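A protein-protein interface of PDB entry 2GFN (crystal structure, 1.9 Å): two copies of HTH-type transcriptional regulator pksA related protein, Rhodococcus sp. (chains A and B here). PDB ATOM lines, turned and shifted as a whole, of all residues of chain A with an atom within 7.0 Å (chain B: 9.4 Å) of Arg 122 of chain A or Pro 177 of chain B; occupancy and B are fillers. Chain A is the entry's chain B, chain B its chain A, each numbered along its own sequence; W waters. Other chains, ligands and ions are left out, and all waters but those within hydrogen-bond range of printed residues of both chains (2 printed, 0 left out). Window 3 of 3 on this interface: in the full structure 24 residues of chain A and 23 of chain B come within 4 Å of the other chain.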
ATOM      1  N   PHE A 111      11.656 -12.184 -15.412  1.00  0.00           N
ATOM      2  CA  PHE A 111      10.605 -12.913 -14.697  1.00  0.00           C
ATOM      3  C   PHE A 111       9.470 -13.466 -15.564  1.00  0.00           C
ATOM      4  O   PHE A 111       8.781 -14.399 -15.163  1.00  0.00           O
ATOM      5  CB  PHE A 111      10.088 -12.133 -13.486  1.00  0.00           C
ATOM      6  CG  PHE A 111      11.010 -12.221 -12.300  1.00  0.00           C
ATOM      7  CD1 PHE A 111      10.993 -13.334 -11.464  1.00  0.00           C
ATOM      8  CD2 PHE A 111      11.934 -11.211 -12.052  1.00  0.00           C
ATOM      9  CE1 PHE A 111      11.890 -13.430 -10.359  1.00  0.00           C
ATOM     10  CE2 PHE A 111      12.815 -11.274 -10.956  1.00  0.00           C
ATOM     11  CZ  PHE A 111      12.801 -12.393 -10.109  1.00  0.00           C
ATOM     12  N   TYR A 112       9.277 -12.882 -16.736  1.00  0.00           N
ATOM     13  CA  TYR A 112       8.415 -13.474 -17.770  1.00  0.00           C
ATOM     14  C   TYR A 112       8.961 -14.837 -18.106  1.00  0.00           C
ATOM     15  O   TYR A 112       8.223 -15.823 -18.142  1.00  0.00           O
ATOM     16  CB  TYR A 112       8.407 -12.633 -19.036  1.00  0.00           C
ATOM     17  CG  TYR A 112       7.395 -11.522 -19.071  1.00  0.00           C
ATOM     18  CD1 TYR A 112       7.208 -10.703 -17.975  1.00  0.00           C
ATOM     19  CD2 TYR A 112       6.682 -11.231 -20.242  1.00  0.00           C
ATOM     20  CE1 TYR A 112       6.297  -9.653 -18.007  1.00  0.00           C
ATOM     21  CE2 TYR A 112       5.778 -10.168 -20.284  1.00  0.00           C
ATOM     22  CZ  TYR A 112       5.604  -9.390 -19.157  1.00  0.00           C
ATOM     23  OH  TYR A 112       4.734  -8.351 -19.162  1.00  0.00           O
ATOM     24  N   GLU A 114      10.943 -16.707 -16.314  1.00  0.00           N
ATOM     25  CA  GLU A 114      10.802 -17.554 -15.131  1.00  0.00           C
ATOM     26  C   GLU A 114       9.356 -17.994 -14.900  1.00  0.00           C
ATOM     27  O   GLU A 114       9.116 -19.141 -14.545  1.00  0.00           O
ATOM     28  CB  GLU A 114      11.296 -16.820 -13.888  1.00  0.00           C
ATOM     29  CG  GLU A 114      11.174 -17.662 -12.624  1.00  0.00           C
ATOM     30  CD  GLU A 114      11.994 -17.122 -11.503  1.00  0.00           C
ATOM     31  OE1 GLU A 114      13.231 -17.016 -11.687  1.00  0.00           O
ATOM     32  OE2 GLU A 114      11.397 -16.802 -10.443  1.00  0.00           O
ATOM     33  N   GLY A 115       8.416 -17.065 -15.085  1.00  0.00           N
ATOM     34  CA  GLY A 115       6.983 -17.318 -14.923  1.00  0.00           C
ATOM     35  C   GLY A 115       6.437 -18.306 -15.943  1.00  0.00           C
ATOM     36  O   GLY A 115       5.396 -18.947 -15.707  1.00  0.00           O
ATOM     37  N   ALA A 116       7.146 -18.440 -17.068  1.00  0.00           N
ATOM     38  CA  ALA A 116       6.819 -19.420 -18.102  1.00  0.00           C
ATOM     39  C   ALA A 116       7.091 -20.833 -17.594  1.00  0.00           C
ATOM     40  O   ALA A 116       6.927 -21.821 -18.331  1.00  0.00           O
ATOM     41  CB  ALA A 116       7.609 -19.136 -19.370  1.00  0.00           C
ATOM     42  N   ALA A 117       7.486 -20.904 -16.322  1.00  0.00           N
ATOM     43  CA  ALA A 117       7.780 -22.153 -15.620  1.00  0.00           C
ATOM     44  C   ALA A 117       7.309 -22.176 -14.154  1.00  0.00           C
ATOM     45  O   ALA A 117       6.757 -23.180 -13.698  1.00  0.00           O
ATOM     46  CB  ALA A 117       9.265 -22.460 -15.709  1.00  0.00           C
ATOM     47  N   GLU A 118       7.517 -21.084 -13.416  1.00  0.00           N
ATOM     48  CA  GLU A 118       7.274 -21.074 -11.961  1.00  0.00           C
ATOM     49  C   GLU A 118       6.087 -20.222 -11.492  1.00  0.00           C
ATOM     50  O   GLU A 118       5.963 -19.039 -11.851  1.00  0.00           O
ATOM     51  CB  GLU A 118       8.542 -20.660 -11.219  1.00  0.00           C
ATOM     52  N   GLU A 119       5.248 -20.821 -10.648  1.00  0.00           N
ATOM     53  CA  GLU A 119       4.008 -20.196 -10.164  1.00  0.00           C
ATOM     54  C   GLU A 119       4.166 -18.874  -9.366  1.00  0.00           C
ATOM     55  O   GLU A 119       3.342 -17.955  -9.509  1.00  0.00           O
ATOM     56  CB  GLU A 119       3.167 -21.230  -9.395  1.00  0.00           C
ATOM     57  CG  GLU A 119       1.812 -20.740  -8.859  1.00  0.00           C
ATOM     58  CD  GLU A 119       0.934 -20.065  -9.906  1.00  0.00           C
ATOM     59  OE1 GLU A 119       0.863 -20.549 -11.056  1.00  0.00           O
ATOM     60  OE2 GLU A 119       0.302 -19.046  -9.563  1.00  0.00           O
ATOM     61  N   THR A 120       5.210 -18.776  -8.546  1.00  0.00           N
ATOM     62  CA  THR A 120       5.456 -17.568  -7.746  1.00  0.00           C
ATOM     63  C   THR A 120       5.660 -16.311  -8.612  1.00  0.00           C
ATOM     64  O   THR A 120       5.008 -15.285  -8.395  1.00  0.00           O
ATOM     65  CB  THR A 120       6.655 -17.754  -6.788  1.00  0.00           C
ATOM     66  OG1 THR A 120       6.538 -16.867  -5.663  1.00  0.00           O
ATOM     67  CG2 THR A 120       8.004 -17.527  -7.515  1.00  0.00           C
ATOM     68  N   ALA A 121       6.563 -16.415  -9.589  1.00  0.00           N
ATOM     69  CA  ALA A 121       6.855 -15.325 -10.527  1.00  0.00           C
ATOM     70  C   ALA A 121       5.676 -15.078 -11.459  1.00  0.00           C
ATOM     71  O   ALA A 121       5.371 -13.929 -11.783  1.00  0.00           O
ATOM     72  CB  ALA A 121       8.131 -15.639 -11.341  1.00  0.00           C
ATOM     73  N   ARG A 122       5.014 -16.151 -11.892  1.00  0.00           N
ATOM     74  CA  ARG A 122       3.856 -16.019 -12.765  1.00  0.00           C
ATOM     75  C   ARG A 122       2.745 -15.162 -12.141  1.00  0.00           C
ATOM     76  O   ARG A 122       2.109 -14.365 -12.829  1.00  0.00           O
ATOM     77  CB  ARG A 122       3.302 -17.386 -13.165  1.00  0.00           C
ATOM     78  CG  ARG A 122       2.518 -17.334 -14.480  1.00  0.00           C
ATOM     79  CD  ARG A 122       1.535 -18.483 -14.609  1.00  0.00           C
ATOM     80  NE  ARG A 122       0.691 -18.584 -13.426  1.00  0.00           N
ATOM     81  CZ  ARG A 122      -0.343 -17.794 -13.153  1.00  0.00           C
ATOM     82  NH1 ARG A 122      -0.710 -16.808 -13.982  1.00  0.00           N
ATOM     83  NH2 ARG A 122      -1.016 -17.995 -12.026  1.00  0.00           N
ATOM     84  N   GLY A 123       2.535 -15.320 -10.839  1.00  0.00           N
ATOM     85  CA  GLY A 123       1.507 -14.576 -10.110  1.00  0.00           C
ATOM     86  C   GLY A 123       1.881 -13.124  -9.875  1.00  0.00           C
ATOM     87  O   GLY A 123       1.006 -12.279  -9.743  1.00  0.00           O
ATOM     88  N   GLU A 124       3.173 -12.830  -9.800  1.00  0.00           N
ATOM     89  CA  GLU A 124       3.639 -11.450  -9.668  1.00  0.00           C
ATOM     90  C   GLU A 124       3.410 -10.727 -10.989  1.00  0.00           C
ATOM     91  O   GLU A 124       2.939  -9.586 -11.003  1.00  0.00           O
ATOM     92  CB  GLU A 124       5.114 -11.397  -9.311  1.00  0.00           C
ATOM     93  CG  GLU A 124       5.389 -11.837  -7.878  1.00  0.00           C
ATOM     94  CD  GLU A 124       5.426 -10.681  -6.913  1.00  0.00           C
ATOM     95  OE1 GLU A 124       4.456  -9.898  -6.799  1.00  0.00           O
ATOM     96  OE2 GLU A 124       6.457 -10.554  -6.258  1.00  0.00           O
ATOM     97  N   ILE A 125       3.724 -11.422 -12.087  1.00  0.00           N
ATOM     98  CA  ILE A 125       3.526 -10.887 -13.440  1.00  0.00           C
ATOM     99  C   ILE A 125       2.042 -10.679 -13.668  1.00  0.00           C
ATOM    100  O   ILE A 125       1.626  -9.622 -14.129  1.00  0.00           O
ATOM    101  CB  ILE A 125       4.089 -11.837 -14.552  1.00  0.00           C
ATOM    102  CG1 ILE A 125       5.608 -12.029 -14.393  1.00  0.00           C
ATOM    103  CG2 ILE A 125       3.727 -11.301 -15.932  1.00  0.00           C
ATOM    104  CD1 ILE A 125       6.361 -10.780 -14.126  1.00  0.00           C
ATOM    105  N   ALA A 126       1.239 -11.680 -13.319  1.00  0.00           N
ATOM    106  CA  ALA A 126      -0.216 -11.546 -13.459  1.00  0.00           C
ATOM    107  C   ALA A 126      -0.804 -10.352 -12.701  1.00  0.00           C
ATOM    108  O   ALA A 126      -1.640  -9.664 -13.262  1.00  0.00           O
ATOM    109  CB  ALA A 126      -0.941 -12.836 -13.085  1.00  0.00           C
ATOM    110  N   ALA A 127      -0.373 -10.108 -11.460  1.00  0.00           N
ATOM    111  CA  ALA A 127      -0.861  -8.938 -10.661  1.00  0.00           C
ATOM    112  C   ALA A 127      -0.498  -7.624 -11.340  1.00  0.00           C
ATOM    113  O   ALA A 127      -1.331  -6.724 -11.444  1.00  0.00           O
ATOM    114  CB  ALA A 127      -0.306  -8.963  -9.223  1.00  0.00           C
ATOM    115  N   ARG A 133      -3.930  -3.186 -16.690  1.00  0.00           N
ATOM    116  CA  ARG A 133      -5.173  -3.187 -17.458  1.00  0.00           C
ATOM    117  C   ARG A 133      -6.276  -2.409 -16.735  1.00  0.00           C
ATOM    118  O   ARG A 133      -7.089  -1.745 -17.365  1.00  0.00           O
ATOM    119  CB  ARG A 133      -5.636  -4.616 -17.756  1.00  0.00           C
ATOM    120  CG  ARG A 133      -4.751  -5.323 -18.800  1.00  0.00           C
ATOM    121  CD  ARG A 133      -5.486  -6.531 -19.413  1.00  0.00           C
ATOM    122  NE  ARG A 133      -5.554  -7.583 -18.401  1.00  0.00           N
ATOM    123  CZ  ARG A 133      -4.631  -8.529 -18.228  1.00  0.00           C
ATOM    124  NH1 ARG A 133      -3.593  -8.632 -19.048  1.00  0.00           N
ATOM    125  NH2 ARG A 133      -4.782  -9.395 -17.253  1.00  0.00           N
ATOM    126  N   ARG B 106       7.552 -20.639 -25.804  1.00  0.00           N
ATOM    127  CA  ARG B 106       8.287 -20.912 -24.573  1.00  0.00           C
ATOM    128  C   ARG B 106       9.782 -20.838 -24.816  1.00  0.00           C
ATOM    129  O   ARG B 106      10.503 -20.217 -24.023  1.00  0.00           O
ATOM    130  CB  ARG B 106       7.905 -22.272 -23.959  1.00  0.00           C
ATOM    131  CG  ARG B 106       6.586 -22.205 -23.132  1.00  0.00           C
ATOM    132  CD  ARG B 106       6.095 -23.580 -22.773  1.00  0.00           C
ATOM    133  NE  ARG B 106       4.890 -23.490 -21.954  1.00  0.00           N
ATOM    134  CZ  ARG B 106       4.171 -24.539 -21.589  1.00  0.00           C
ATOM    135  NH1 ARG B 106       4.538 -25.758 -21.984  1.00  0.00           N
ATOM    136  NH2 ARG B 106       3.078 -24.358 -20.854  1.00  0.00           N
ATOM    137  N   LEU B 109      10.816 -17.171 -25.602  1.00  0.00           N
ATOM    138  CA  LEU B 109      10.805 -16.360 -24.365  1.00  0.00           C
ATOM    139  C   LEU B 109      12.054 -16.623 -23.510  1.00  0.00           C
ATOM    140  O   LEU B 109      12.700 -15.668 -23.040  1.00  0.00           O
ATOM    141  CB  LEU B 109       9.521 -16.609 -23.569  1.00  0.00           C
ATOM    142  CG  LEU B 109       9.321 -15.787 -22.277  1.00  0.00           C
ATOM    143  CD1 LEU B 109       9.758 -14.350 -22.485  1.00  0.00           C
ATOM    144  CD2 LEU B 109       7.864 -15.875 -21.826  1.00  0.00           C
ATOM    145  N   LEU B 169       0.928 -10.282 -27.115  1.00  0.00           N
ATOM    146  CA  LEU B 169      -0.177 -11.181 -26.839  1.00  0.00           C
ATOM    147  C   LEU B 169       0.305 -12.601 -26.618  1.00  0.00           C
ATOM    148  O   LEU B 169      -0.139 -13.304 -25.674  1.00  0.00           O
ATOM    149  CB  LEU B 169      -1.222 -11.184 -27.999  1.00  0.00           C
ATOM    150  CG  LEU B 169      -2.131  -9.941 -28.066  1.00  0.00           C
ATOM    151  CD1 LEU B 169      -2.934  -9.982 -29.314  1.00  0.00           C
ATOM    152  CD2 LEU B 169      -3.095  -9.807 -26.830  1.00  0.00           C
ATOM    153  N   LEU B 171       3.240 -13.628 -25.643  1.00  0.00           N
ATOM    154  CA  LEU B 171       4.044 -13.765 -24.431  1.00  0.00           C
ATOM    155  C   LEU B 171       3.204 -13.669 -23.177  1.00  0.00           C
ATOM    156  O   LEU B 171       3.392 -14.492 -22.265  1.00  0.00           O
ATOM    157  CB  LEU B 171       5.237 -12.769 -24.368  1.00  0.00           C
ATOM    158  CG  LEU B 171       6.243 -12.856 -25.533  1.00  0.00           C
ATOM    159  CD1 LEU B 171       7.294 -11.756 -25.427  1.00  0.00           C
ATOM    160  CD2 LEU B 171       6.954 -14.221 -25.623  1.00  0.00           C
ATOM    161  N   GLN B 172       2.296 -12.685 -23.114  1.00  0.00           N
ATOM    162  CA  GLN B 172       1.386 -12.551 -21.966  1.00  0.00           C
ATOM    163  C   GLN B 172       0.498 -13.773 -21.863  1.00  0.00           C
ATOM    164  O   GLN B 172       0.150 -14.227 -20.748  1.00  0.00           O
ATOM    165  CB  GLN B 172       0.544 -11.285 -22.084  1.00  0.00           C
ATOM    166  CG  GLN B 172       1.394 -10.004 -21.881  1.00  0.00           C
ATOM    167  CD  GLN B 172       0.598  -8.724 -22.058  1.00  0.00           C
ATOM    168  OE1 GLN B 172      -0.615  -8.750 -22.303  1.00  0.00           O
ATOM    169  NE2 GLN B 172       1.268  -7.605 -21.944  1.00  0.00           N
ATOM    170  N   ALA B 173       0.113 -14.310 -23.010  1.00  0.00           N
ATOM    171  CA  ALA B 173      -0.835 -15.419 -22.984  1.00  0.00           C
ATOM    172  C   ALA B 173      -0.286 -16.632 -22.243  1.00  0.00           C
ATOM    173  O   ALA B 173      -1.081 -17.350 -21.635  1.00  0.00           O
ATOM    174  CB  ALA B 173      -1.335 -15.798 -24.388  1.00  0.00           C
ATOM    175  N   ILE B 174       1.033 -16.860 -22.260  1.00  0.00           N
ATOM    176  CA  ILE B 174       1.596 -18.075 -21.597  1.00  0.00           C
ATOM    177  C   ILE B 174       1.774 -17.865 -20.084  1.00  0.00           C
ATOM    178  O   ILE B 174       2.044 -18.797 -19.347  1.00  0.00           O
ATOM    179  CB  ILE B 174       2.845 -18.728 -22.325  1.00  0.00           C
ATOM    180  CG1 ILE B 174       4.104 -17.858 -22.231  1.00  0.00           C
ATOM    181  CG2 ILE B 174       2.531 -19.098 -23.796  1.00  0.00           C
ATOM    182  CD1 ILE B 174       5.387 -18.582 -22.703  1.00  0.00           C
ATOM    183  N   LEU B 175       1.585 -16.618 -19.648  1.00  0.00           N
ATOM    184  CA  LEU B 175       1.681 -16.203 -18.254  1.00  0.00           C
ATOM    185  C   LEU B 175       0.327 -15.885 -17.627  1.00  0.00           C
ATOM    186  O   LEU B 175       0.147 -16.014 -16.414  1.00  0.00           O
ATOM    187  CB  LEU B 175       2.582 -14.972 -18.166  1.00  0.00           C
ATOM    188  CG  LEU B 175       3.994 -15.226 -18.732  1.00  0.00           C
ATOM    189  CD1 LEU B 175       4.832 -13.964 -18.880  1.00  0.00           C
ATOM    190  CD2 LEU B 175       4.716 -16.257 -17.879  1.00  0.00           C
ATOM    191  N   ASP B 176      -0.631 -15.479 -18.450  1.00  0.00           N
ATOM    192  CA  ASP B 176      -1.837 -14.832 -17.947  1.00  0.00           C
ATOM    193  C   ASP B 176      -3.045 -15.374 -18.677  1.00  0.00           C
ATOM    194  O   ASP B 176      -3.265 -15.028 -19.821  1.00  0.00           O
ATOM    195  CB  ASP B 176      -1.729 -13.309 -18.171  1.00  0.00           C
ATOM    196  CG  ASP B 176      -2.876 -12.515 -17.527  1.00  0.00           C
ATOM    197  OD1 ASP B 176      -3.930 -13.105 -17.190  1.00  0.00           O
ATOM    198  OD2 ASP B 176      -2.728 -11.276 -17.392  1.00  0.00           O
ATOM    199  N   PRO B 177      -3.869 -16.192 -17.997  1.00  0.00           N
ATOM    200  CA  PRO B 177      -5.032 -16.822 -18.633  1.00  0.00           C
ATOM    201  C   PRO B 177      -6.058 -15.823 -19.171  1.00  0.00           C
ATOM    202  O   PRO B 177      -6.792 -16.169 -20.091  1.00  0.00           O
ATOM    203  CB  PRO B 177      -5.638 -17.685 -17.528  1.00  0.00           C
ATOM    204  CG  PRO B 177      -5.057 -17.201 -16.261  1.00  0.00           C
ATOM    205  CD  PRO B 177      -3.724 -16.575 -16.585  1.00  0.00           C
ATOM    206  N   VAL B 178      -6.087 -14.596 -18.639  1.00  0.00           N
ATOM    207  CA  VAL B 178      -6.950 -13.513 -19.192  1.00  0.00           C
ATOM    208  C   VAL B 178      -6.605 -13.281 -20.683  1.00  0.00           C
ATOM    209  O   VAL B 178      -7.478 -13.203 -21.532  1.00  0.00           O
ATOM    210  CB  VAL B 178      -6.815 -12.164 -18.418  1.00  0.00           C
ATOM    211  CG1 VAL B 178      -7.657 -11.053 -19.074  1.00  0.00           C
ATOM    212  CG2 VAL B 178      -7.215 -12.317 -16.951  1.00  0.00           C
ATOM    213  N   VAL B 179      -5.315 -13.189 -20.985  1.00  0.00           N
ATOM    214  CA  VAL B 179      -4.876 -12.952 -22.348  1.00  0.00           C
ATOM    215  C   VAL B 179      -4.979 -14.256 -23.154  1.00  0.00           C
ATOM    216  O   VAL B 179      -5.298 -14.226 -24.340  1.00  0.00           O
ATOM    217  CB  VAL B 179      -3.426 -12.418 -22.384  1.00  0.00           C
ATOM    218  CG1 VAL B 179      -2.966 -12.147 -23.838  1.00  0.00           C
ATOM    219  CG2 VAL B 179      -3.277 -11.157 -21.519  1.00  0.00           C
ATOM    220  N   MET B 180      -4.725 -15.401 -22.517  1.00  0.00           N
ATOM    221  CA  MET B 180      -4.884 -16.692 -23.223  1.00  0.00           C
ATOM    222  C   MET B 180      -6.337 -16.847 -23.719  1.00  0.00           C
ATOM    223  O   MET B 180      -6.576 -17.245 -24.867  1.00  0.00           O
ATOM    224  CB  MET B 180      -4.500 -17.885 -22.341  1.00  0.00           C
ATOM    225  CG  MET B 180      -4.668 -19.260 -23.069  1.00  0.00           C
ATOM    226  SD  MET B 180      -3.609 -19.474 -24.732  1.00  0.00           S
ATOM    227  CE  MET B 180      -1.906 -19.939 -23.941  1.00  0.00           C
ATOM    228  N   LYS B 181      -7.296 -16.521 -22.847  1.00  0.00           N
ATOM    229  CA  LYS B 181      -8.714 -16.457 -23.250  1.00  0.00           C
ATOM    230  C   LYS B 181      -8.924 -15.504 -24.430  1.00  0.00           C
ATOM    231  O   LYS B 181      -9.523 -15.884 -25.437  1.00  0.00           O
ATOM    232  CB  LYS B 181      -9.607 -16.046 -22.079  1.00  0.00           C
ATOM    233  CG  LYS B 181     -11.094 -15.974 -22.455  1.00  0.00           C
ATOM    234  CD  LYS B 181     -12.010 -15.592 -21.283  1.00  0.00           C
ATOM    235  CE  LYS B 181     -13.403 -16.232 -21.484  1.00  0.00           C
ATOM    236  NZ  LYS B 181     -14.255 -16.331 -20.225  1.00  0.00           N
ATOM    237  N   ALA B 182      -8.415 -14.278 -24.310  1.00  0.00           N
ATOM    238  CA  ALA B 182      -8.536 -13.292 -25.356  1.00  0.00           C
ATOM    239  C   ALA B 182      -8.076 -13.805 -26.744  1.00  0.00           C
ATOM    240  O   ALA B 182      -8.800 -13.657 -27.733  1.00  0.00           O
ATOM    241  CB  ALA B 182      -7.779 -12.010 -24.953  1.00  0.00           C
ATOM    242  N   ILE B 183      -6.887 -14.407 -26.818  1.00  0.00           N
ATOM    243  CA  ILE B 183      -6.335 -14.846 -28.117  1.00  0.00           C
ATOM    244  C   ILE B 183      -6.919 -16.150 -28.646  1.00  0.00           C
ATOM    245  O   ILE B 183      -6.680 -16.503 -29.795  1.00  0.00           O
ATOM    246  CB  ILE B 183      -4.788 -14.950 -28.122  1.00  0.00           C
ATOM    247  CG1 ILE B 183      -4.273 -16.043 -27.171  1.00  0.00           C
ATOM    248  CG2 ILE B 183      -4.155 -13.572 -27.848  1.00  0.00           C
ATOM    249  CD1 ILE B 183      -2.866 -16.482 -27.533  1.00  0.00           C
ATOM    250  N   SER B 184      -7.678 -16.840 -27.805  1.00  0.00           N
ATOM    251  CA  SER B 184      -8.373 -18.075 -28.196  1.00  0.00           C
ATOM    252  C   SER B 184      -9.701 -17.809 -28.926  1.00  0.00           C
ATOM    253  O   SER B 184     -10.328 -18.737 -29.451  1.00  0.00           O
ATOM    254  CB  SER B 184      -8.580 -18.967 -26.959  1.00  0.00           C
ATOM    255  OG  SER B 184      -7.312 -19.289 -26.378  1.00  0.00           O
HETATM  256  O   HOH W   1      -3.596 -10.860 -14.639  1.00  0.00           O
HETATM  257  O   HOH W   2       4.421 -21.229 -20.048  1.00  0.00           O
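Water W1 lies within hydrogen-bond range of the backbone carbonyl oxygen (O) of Ala 126 of chain A (2.7 Å), the side-chain carboxylate (OD2) of Asp 176 of chain B (2.9 Å) and the guanidinium group (NH2) of Arg 133 of chain A (3.2 Å).
Water W2 lies within hydrogen-bond range of the guanidinium group of Arg 106 of chain B (3.0 Å), the backbone carbonyl oxygen of Ala 116 of chain A (3.1 Å) and the backbone carbonyl oxygen of Ile 174 of chain B (3.5 Å).
OD1 of Asp 176 of chain B lies within hydrogen-bond range of N of Val 178 of chain B (3.0 Å).
OE2 of Glu 119 of chain A lies within salt-bridge range of NH2 of Arg 122 of chain A (3.0 Å).
Of the 17 printed residues of chain B, 6 touch a printed residue of chain A.
Hydrophobic or aromatic side chains of chain B within 4 Å of the printed part of chain A: Leu 109, Leu 175, Pro 177, Val 178 and Val 179.
Hydrophobic or aromatic side chains of chain A that line the printed part of chain B: Tyr 112.
No position is printed for both chains.
CD2 of Leu 109 of chain B touches O of Tyr 112 of chain A (3.7 Å).
Tyr 112 of chain A touches Leu 175 of chain B (O to CD2, 3.5 Å).
Gly 115 of chain A touches Leu 175 of chain B.
Ala 116 of chain A touches Leu 175 of chain B.
NH1 of Arg 122 of chain A touches CD of Pro 177 of chain B, 3.99 Å away.
Arg 133 of chain A touches Val 178 of chain B.
NH1 of Arg 133 of chain A touches CG2 of Val 179 of chain B, 3.5 Å away.
Of the printed residues of chain B, Tyr 112 of chain A touches Leu 109 (3.7 Å) and Leu 175 (3.5 Å).
Of chain B, only Leu 175 comes within 4 Å of Gly 115 of chain A.
No residue of chain B comes within 4 Å of Gly 123 of chain A.
Of the printed residues of chain B, Arg 133 of chain A touches Asp 176 (2.8 Å), Val 178 (3.6 Å) and Val 179 (3.5 Å).
Of the printed residues of chain A, Leu 175 of chain B touches Tyr 112, Gly 115, Ala 116 and Arg 122.
Of the printed residues of chain A, Pro 177 of chain B touches Arg 122.
Printed residues of chain A within 4 Å of Val 179 of chain B: Arg 133 (3.5 Å).
The nearest printed residue of chain B that does not touch Arg 122 of chain A is Asp 176 of chain B (4.6 Å).
The nearest printed residue of chain A that does not touch Pro 177 of chain B is Ala 126 of chain A (5.8 Å).
NH2 of Arg 133 of chain A lies within salt-bridge range of OD2 of Asp 176 of chain B (2.8 Å).
The guanidinium group of Arg 122 of chain A sits at hydrogen-bond distance from the backbone carbonyl oxygen of Leu 175 of chain B.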
